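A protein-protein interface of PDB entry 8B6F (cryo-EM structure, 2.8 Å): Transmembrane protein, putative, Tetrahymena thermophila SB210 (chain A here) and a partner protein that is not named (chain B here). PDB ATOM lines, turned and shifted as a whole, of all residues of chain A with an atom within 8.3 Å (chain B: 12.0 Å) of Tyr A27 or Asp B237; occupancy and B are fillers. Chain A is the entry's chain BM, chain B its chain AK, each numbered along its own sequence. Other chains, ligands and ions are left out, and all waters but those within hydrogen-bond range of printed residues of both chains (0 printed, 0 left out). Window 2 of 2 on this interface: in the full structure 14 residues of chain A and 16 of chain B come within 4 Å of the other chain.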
ATOM      1  N   HIS A  23      15.293  22.020  13.615  1.00  0.00           N
ATOM      2  CA  HIS A  23      14.904  21.037  14.617  1.00  0.00           C
ATOM      3  C   HIS A  23      14.823  21.623  16.020  1.00  0.00           C
ATOM      4  O   HIS A  23      14.329  20.943  16.925  1.00  0.00           O
ATOM      5  CB  HIS A  23      15.891  19.870  14.615  1.00  0.00           C
ATOM      6  CG  HIS A  23      17.270  20.248  15.058  1.00  0.00           C
ATOM      7  ND1 HIS A  23      18.129  20.989  14.274  1.00  0.00           N
ATOM      8  CD2 HIS A  23      17.940  19.986  16.204  1.00  0.00           C
ATOM      9  CE1 HIS A  23      19.266  21.168  14.919  1.00  0.00           C
ATOM     10  NE2 HIS A  23      19.179  20.568  16.092  1.00  0.00           N
ATOM     11  N   ARG A  24      15.305  22.845  16.228  1.00  0.00           N
ATOM     12  CA  ARG A  24      15.290  23.478  17.544  1.00  0.00           C
ATOM     13  C   ARG A  24      13.974  24.225  17.690  1.00  0.00           C
ATOM     14  O   ARG A  24      13.799  25.313  17.138  1.00  0.00           O
ATOM     15  CB  ARG A  24      16.482  24.413  17.704  1.00  0.00           C
ATOM     16  CG  ARG A  24      17.826  23.751  17.442  1.00  0.00           C
ATOM     17  CD  ARG A  24      18.938  24.775  17.309  1.00  0.00           C
ATOM     18  NE  ARG A  24      18.682  25.711  16.222  1.00  0.00           N
ATOM     19  CZ  ARG A  24      19.523  26.658  15.832  1.00  0.00           C
ATOM     20  NH1 ARG A  24      20.700  26.819  16.411  1.00  0.00           N
ATOM     21  NH2 ARG A  24      19.176  27.461  14.830  1.00  0.00           N
ATOM     22  N   GLN A  25      13.044  23.645  18.442  1.00  0.00           N
ATOM     23  CA  GLN A  25      11.742  24.244  18.678  1.00  0.00           C
ATOM     24  C   GLN A  25      11.469  24.292  20.173  1.00  0.00           C
ATOM     25  O   GLN A  25      11.908  23.410  20.915  1.00  0.00           O
ATOM     26  CB  GLN A  25      10.630  23.446  17.983  1.00  0.00           C
ATOM     27  CG  GLN A  25      10.774  23.360  16.475  1.00  0.00           C
ATOM     28  CD  GLN A  25      10.576  24.697  15.792  1.00  0.00           C
ATOM     29  OE1 GLN A  25      10.241  25.691  16.432  1.00  0.00           O
ATOM     30  NE2 GLN A  25      10.781  24.725  14.481  1.00  0.00           N
ATOM     31  N   PRO A  26      10.745  25.307  20.645  1.00  0.00           N
ATOM     32  CA  PRO A  26      10.431  25.371  22.077  1.00  0.00           C
ATOM     33  C   PRO A  26       9.568  24.195  22.509  1.00  0.00           C
ATOM     34  O   PRO A  26       8.738  23.690  21.749  1.00  0.00           O
ATOM     35  CB  PRO A  26       9.689  26.705  22.222  1.00  0.00           C
ATOM     36  CG  PRO A  26       9.175  27.012  20.865  1.00  0.00           C
ATOM     37  CD  PRO A  26      10.164  26.438  19.902  1.00  0.00           C
ATOM     38  N   TYR A  27       9.776  23.757  23.751  1.00  0.00           N
ATOM     39  CA  TYR A  27       9.050  22.595  24.253  1.00  0.00           C
ATOM     40  C   TYR A  27       7.551  22.859  24.311  1.00  0.00           C
ATOM     41  O   TYR A  27       6.747  21.989  23.959  1.00  0.00           O
ATOM     42  CB  TYR A  27       9.579  22.203  25.632  1.00  0.00           C
ATOM     43  CG  TYR A  27       9.232  23.187  26.722  1.00  0.00           C
ATOM     44  CD1 TYR A  27      10.023  24.301  26.953  1.00  0.00           C
ATOM     45  CD2 TYR A  27       8.117  22.996  27.525  1.00  0.00           C
ATOM     46  CE1 TYR A  27       9.712  25.200  27.948  1.00  0.00           C
ATOM     47  CE2 TYR A  27       7.796  23.888  28.522  1.00  0.00           C
ATOM     48  CZ  TYR A  27       8.599  24.987  28.729  1.00  0.00           C
ATOM     49  OH  TYR A  27       8.284  25.875  29.723  1.00  0.00           O
ATOM     50  N   ASP A  28       7.155  24.052  24.749  1.00  0.00           N
ATOM     51  CA  ASP A  28       5.747  24.373  24.934  1.00  0.00           C
ATOM     52  C   ASP A  28       5.033  24.679  23.626  1.00  0.00           C
ATOM     53  O   ASP A  28       3.852  25.036  23.655  1.00  0.00           O
ATOM     54  CB  ASP A  28       5.592  25.556  25.893  1.00  0.00           C
ATOM     55  CG  ASP A  28       6.197  26.827  25.350  1.00  0.00           C
ATOM     56  OD1 ASP A  28       7.137  26.736  24.537  1.00  0.00           O
ATOM     57  OD2 ASP A  28       5.736  27.919  25.740  1.00  0.00           O
ATOM     58  N   LEU A  29       5.713  24.568  22.488  1.00  0.00           N
ATOM     59  CA  LEU A  29       5.020  24.666  21.214  1.00  0.00           C
ATOM     60  C   LEU A  29       3.930  23.607  21.151  1.00  0.00           C
ATOM     61  O   LEU A  29       4.141  22.451  21.527  1.00  0.00           O
ATOM     62  CB  LEU A  29       6.004  24.488  20.058  1.00  0.00           C
ATOM     63  CG  LEU A  29       5.438  24.686  18.650  1.00  0.00           C
ATOM     64  CD1 LEU A  29       5.054  26.138  18.420  1.00  0.00           C
ATOM     65  CD2 LEU A  29       6.434  24.223  17.603  1.00  0.00           C
ATOM     66  N   ASN A  30       2.750  24.014  20.690  1.00  0.00           N
ATOM     67  CA  ASN A  30       1.560  23.177  20.591  1.00  0.00           C
ATOM     68  C   ASN A  30       0.917  22.912  21.943  1.00  0.00           C
ATOM     69  O   ASN A  30       0.011  22.074  22.032  1.00  0.00           O
ATOM     70  CB  ASN A  30       1.856  21.834  19.914  1.00  0.00           C
ATOM     71  CG  ASN A  30       2.551  21.993  18.579  1.00  0.00           C
ATOM     72  OD1 ASN A  30       2.346  22.979  17.873  1.00  0.00           O
ATOM     73  ND2 ASN A  30       3.381  21.020  18.226  1.00  0.00           N
ATOM     74  N   PHE A  31       1.356  23.586  23.002  1.00  0.00           N
ATOM     75  CA  PHE A  31       0.679  23.451  24.280  1.00  0.00           C
ATOM     76  C   PHE A  31      -0.687  24.124  24.226  1.00  0.00           C
ATOM     77  O   PHE A  31      -0.950  25.007  23.407  1.00  0.00           O
ATOM     78  CB  PHE A  31       1.506  24.063  25.413  1.00  0.00           C
ATOM     79  CG  PHE A  31       2.504  23.121  26.031  1.00  0.00           C
ATOM     80  CD1 PHE A  31       2.907  21.966  25.377  1.00  0.00           C
ATOM     81  CD2 PHE A  31       3.037  23.394  27.280  1.00  0.00           C
ATOM     82  CE1 PHE A  31       3.823  21.109  25.956  1.00  0.00           C
ATOM     83  CE2 PHE A  31       3.951  22.541  27.863  1.00  0.00           C
ATOM     84  CZ  PHE A  31       4.346  21.398  27.201  1.00  0.00           C
ATOM     85  N   ASN A  34      -0.777  27.985  24.780  1.00  0.00           N
ATOM     86  CA  ASN A  34      -0.315  28.808  23.672  1.00  0.00           C
ATOM     87  C   ASN A  34      -1.378  29.008  22.600  1.00  0.00           C
ATOM     88  O   ASN A  34      -1.151  29.787  21.671  1.00  0.00           O
ATOM     89  CB  ASN A  34       0.931  28.184  23.042  1.00  0.00           C
ATOM     90  CG  ASN A  34       2.135  28.245  23.955  1.00  0.00           C
ATOM     91  OD1 ASN A  34       2.248  29.137  24.792  1.00  0.00           O
ATOM     92  ND2 ASN A  34       3.046  27.293  23.797  1.00  0.00           N
ATOM     93  N   PRO B 232      12.727  16.614  10.500  1.00  0.00           N
ATOM     94  CA  PRO B 232      13.637  16.091  11.524  1.00  0.00           C
ATOM     95  C   PRO B 232      13.038  14.900  12.257  1.00  0.00           C
ATOM     96  O   PRO B 232      11.827  14.814  12.467  1.00  0.00           O
ATOM     97  CB  PRO B 232      13.839  17.282  12.469  1.00  0.00           C
ATOM     98  CG  PRO B 232      13.443  18.478  11.682  1.00  0.00           C
ATOM     99  CD  PRO B 232      12.368  18.018  10.755  1.00  0.00           C
ATOM    100  N   THR B 233      13.911  13.971  12.651  1.00  0.00           N
ATOM    101  CA  THR B 233      13.460  12.821  13.426  1.00  0.00           C
ATOM    102  C   THR B 233      13.108  13.220  14.853  1.00  0.00           C
ATOM    103  O   THR B 233      12.074  12.798  15.386  1.00  0.00           O
ATOM    104  CB  THR B 233      14.539  11.737  13.429  1.00  0.00           C
ATOM    105  OG1 THR B 233      14.858  11.369  12.081  1.00  0.00           O
ATOM    106  CG2 THR B 233      14.065  10.503  14.188  1.00  0.00           C
ATOM    107  N   LYS B 234      13.951  14.034  15.486  1.00  0.00           N
ATOM    108  CA  LYS B 234      13.737  14.494  16.848  1.00  0.00           C
ATOM    109  C   LYS B 234      13.971  15.994  16.914  1.00  0.00           C
ATOM    110  O   LYS B 234      14.733  16.554  16.123  1.00  0.00           O
ATOM    111  CB  LYS B 234      14.663  13.776  17.836  1.00  0.00           C
ATOM    112  CG  LYS B 234      16.140  13.896  17.494  1.00  0.00           C
ATOM    113  CD  LYS B 234      17.003  13.053  18.422  1.00  0.00           C
ATOM    114  CE  LYS B 234      17.038  13.608  19.840  1.00  0.00           C
ATOM    115  NZ  LYS B 234      17.655  14.962  19.904  1.00  0.00           N
ATOM    116  N   TYR B 235      13.312  16.639  17.870  1.00  0.00           N
ATOM    117  CA  TYR B 235      13.387  18.081  18.046  1.00  0.00           C
ATOM    118  C   TYR B 235      14.050  18.418  19.374  1.00  0.00           C
ATOM    119  O   TYR B 235      13.930  17.679  20.356  1.00  0.00           O
ATOM    120  CB  TYR B 235      11.995  18.716  17.986  1.00  0.00           C
ATOM    121  CG  TYR B 235      11.361  18.652  16.618  1.00  0.00           C
ATOM    122  CD1 TYR B 235      10.708  17.506  16.186  1.00  0.00           C
ATOM    123  CD2 TYR B 235      11.411  19.741  15.760  1.00  0.00           C
ATOM    124  CE1 TYR B 235      10.126  17.446  14.934  1.00  0.00           C
ATOM    125  CE2 TYR B 235      10.834  19.691  14.508  1.00  0.00           C
ATOM    126  CZ  TYR B 235      10.191  18.542  14.101  1.00  0.00           C
ATOM    127  OH  TYR B 235       9.616  18.490  12.853  1.00  0.00           O
ATOM    128  N   ASP B 236      14.755  19.545  19.390  1.00  0.00           N
ATOM    129  CA  ASP B 236      15.442  20.041  20.571  1.00  0.00           C
ATOM    130  C   ASP B 236      14.785  21.325  21.055  1.00  0.00           C
ATOM    131  O   ASP B 236      14.027  21.975  20.330  1.00  0.00           O
ATOM    132  CB  ASP B 236      16.924  20.297  20.281  1.00  0.00           C
ATOM    133  CG  ASP B 236      17.668  19.039  19.884  1.00  0.00           C
ATOM    134  OD1 ASP B 236      17.343  17.959  20.419  1.00  0.00           O
ATOM    135  OD2 ASP B 236      18.583  19.129  19.040  1.00  0.00           O
ATOM    136  N   ASP B 237      15.081  21.683  22.300  1.00  0.00           N
ATOM    137  CA  ASP B 237      14.572  22.911  22.892  1.00  0.00           C
ATOM    138  C   ASP B 237      15.492  24.074  22.544  1.00  0.00           C
ATOM    139  O   ASP B 237      16.718  23.952  22.609  1.00  0.00           O
ATOM    140  CB  ASP B 237      14.450  22.771  24.410  1.00  0.00           C
ATOM    141  CG  ASP B 237      13.725  23.939  25.045  1.00  0.00           C
ATOM    142  OD1 ASP B 237      12.531  24.134  24.743  1.00  0.00           O
ATOM    143  OD2 ASP B 237      14.346  24.663  25.850  1.00  0.00           O
ATOM    144  N   VAL B 238      14.893  25.199  22.164  1.00  0.00           N
ATOM    145  CA  VAL B 238      15.664  26.372  21.763  1.00  0.00           C
ATOM    146  C   VAL B 238      16.357  26.940  22.999  1.00  0.00           C
ATOM    147  O   VAL B 238      15.708  27.465  23.907  1.00  0.00           O
ATOM    148  CB  VAL B 238      14.782  27.421  21.072  1.00  0.00           C
ATOM    149  CG1 VAL B 238      14.182  26.849  19.800  1.00  0.00           C
ATOM    150  CG2 VAL B 238      13.668  27.923  21.988  1.00  0.00           C
ATOM    151  N   THR B 239      17.682  26.802  23.052  1.00  0.00           N
ATOM    152  CA  THR B 239      18.484  27.350  24.140  1.00  0.00           C
ATOM    153  C   THR B 239      19.178  28.645  23.733  1.00  0.00           C
ATOM    154  O   THR B 239      18.920  29.702  24.314  1.00  0.00           O
ATOM    155  CB  THR B 239      19.521  26.317  24.602  1.00  0.00           C
ATOM    156  OG1 THR B 239      20.404  25.997  23.518  1.00  0.00           O
ATOM    157  CG2 THR B 239      18.836  25.051  25.088  1.00  0.00           C
ATOM    158  N   ILE B 240      20.052  28.581  22.735  1.00  0.00           N
ATOM    159  CA  ILE B 240      20.769  29.757  22.259  1.00  0.00           C
ATOM    160  C   ILE B 240      21.342  29.431  20.889  1.00  0.00           C
ATOM    161  O   ILE B 240      21.777  28.306  20.635  1.00  0.00           O
ATOM    162  CB  ILE B 240      21.872  30.184  23.259  1.00  0.00           C
ATOM    163  CG1 ILE B 240      22.564  31.472  22.802  1.00  0.00           C
ATOM    164  CG2 ILE B 240      22.905  29.080  23.422  1.00  0.00           C
ATOM    165  CD1 ILE B 240      21.673  32.686  22.824  1.00  0.00           C
ATOM    166  N   ASN B 241      21.343  30.427  20.009  1.00  0.00           N
ATOM    167  CA  ASN B 241      21.941  30.289  18.690  1.00  0.00           C
ATOM    168  C   ASN B 241      23.413  30.658  18.779  1.00  0.00           C
ATOM    169  O   ASN B 241      23.763  31.715  19.311  1.00  0.00           O
ATOM    170  CB  ASN B 241      21.233  31.181  17.673  1.00  0.00           C
ATOM    171  CG  ASN B 241      19.837  30.701  17.349  1.00  0.00           C
ATOM    172  OD1 ASN B 241      19.278  29.860  18.051  1.00  0.00           O
ATOM    173  ND2 ASN B 241      19.260  31.240  16.284  1.00  0.00           N
ATOM    174  N   TYR B 242      24.274  29.782  18.260  1.00  0.00           N
ATOM    175  CA  TYR B 242      25.705  30.039  18.345  1.00  0.00           C
ATOM    176  C   TYR B 242      26.071  31.372  17.710  1.00  0.00           C
ATOM    177  O   TYR B 242      27.036  32.016  18.134  1.00  0.00           O
ATOM    178  CB  TYR B 242      26.488  28.903  17.687  1.00  0.00           C
ATOM    179  CG  TYR B 242      26.441  28.920  16.179  1.00  0.00           C
ATOM    180  CD1 TYR B 242      25.338  28.433  15.492  1.00  0.00           C
ATOM    181  CD2 TYR B 242      27.505  29.419  15.442  1.00  0.00           C
ATOM    182  CE1 TYR B 242      25.295  28.450  14.113  1.00  0.00           C
ATOM    183  CE2 TYR B 242      27.472  29.440  14.065  1.00  0.00           C
ATOM    184  CZ  TYR B 242      26.365  28.953  13.406  1.00  0.00           C
ATOM    185  OH  TYR B 242      26.332  28.972  12.033  1.00  0.00           O
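The backbone NH of Asp B236 lies within hydrogen-bond range of the backbone carbonyl oxygen of His A23, at 2.9 Å.
N of Gln A25 lies within hydrogen-bond range of O of Asp B236, at 2.7 Å.
The side-chain carboxylate (OD1) of Asp B237 lies within hydrogen-bond range of the backbone NH (N) of Tyr A27 (3.0 Å).
The side-chain amino group (NZ) of Lys B234 lies within salt-bridge range of the side-chain carboxylate (OD1) of Asp B236, 3.1 Å away.
Among the printed residues, merely in contact across the chains: His A23 with Pro B232 (3.9 Å), His A23 with Lys B234 (3.8 Å), His A23 with Tyr B235 (3.2 Å), Arg A24 with Asp B236 (3.4 Å), Arg A24 with Val B238 (3.1 Å), Arg A24 with Asn B241 (3.7 Å), Gln A25 with Tyr B235 (3.7 Å), Gln A25 with Asp B237 (3.4 Å), Gln A25 with Val B238 (3.7 Å), Pro A26 with Asp B237 (3.6 Å) and Pro A26 with Val B238 (3.9 Å).
Tyr A27 touches just one residue of chain B: Asp B237 (3.0 Å).
Of chain A, only Gln A25 (3.4 Å), Pro A26 (3.6 Å) and Tyr A27 (3.0 Å) come within 4 Å of Asp B237.
Pro A26 touches just these residues of chain B: Asp B237 and Val B238.
No residue of chain B comes within 4 Å of Asp A28.
No residue of chain B comes within 4 Å of Leu A29.
Printed residues of chain A within 4 Å of Lys B234: His A23 (3.8 Å).
Of the printed residues of chain A, Asp B236 touches His A23, Arg A24 and Gln A25.
Of the printed residues of chain A, Val B238 touches Arg A24 (3.1 Å), Gln A25 (3.7 Å) and Pro A26 (3.9 Å).
Thr B239 touches none of the printed residues of chain A.
Tyr B242 touches none of the printed residues of chain A.
The nearest residue of chain B that does not touch Tyr A27 is Val B238 (5.5 Å).
Hydrophobic or aromatic side chains of chain B within 4 Å of the printed part of chain A: Pro B232, Tyr B235 and Val B238.
Printed residues of chain A that touch a printed residue of chain B: His A23, Arg A24, Gln A25, Pro A26 and Tyr A27.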
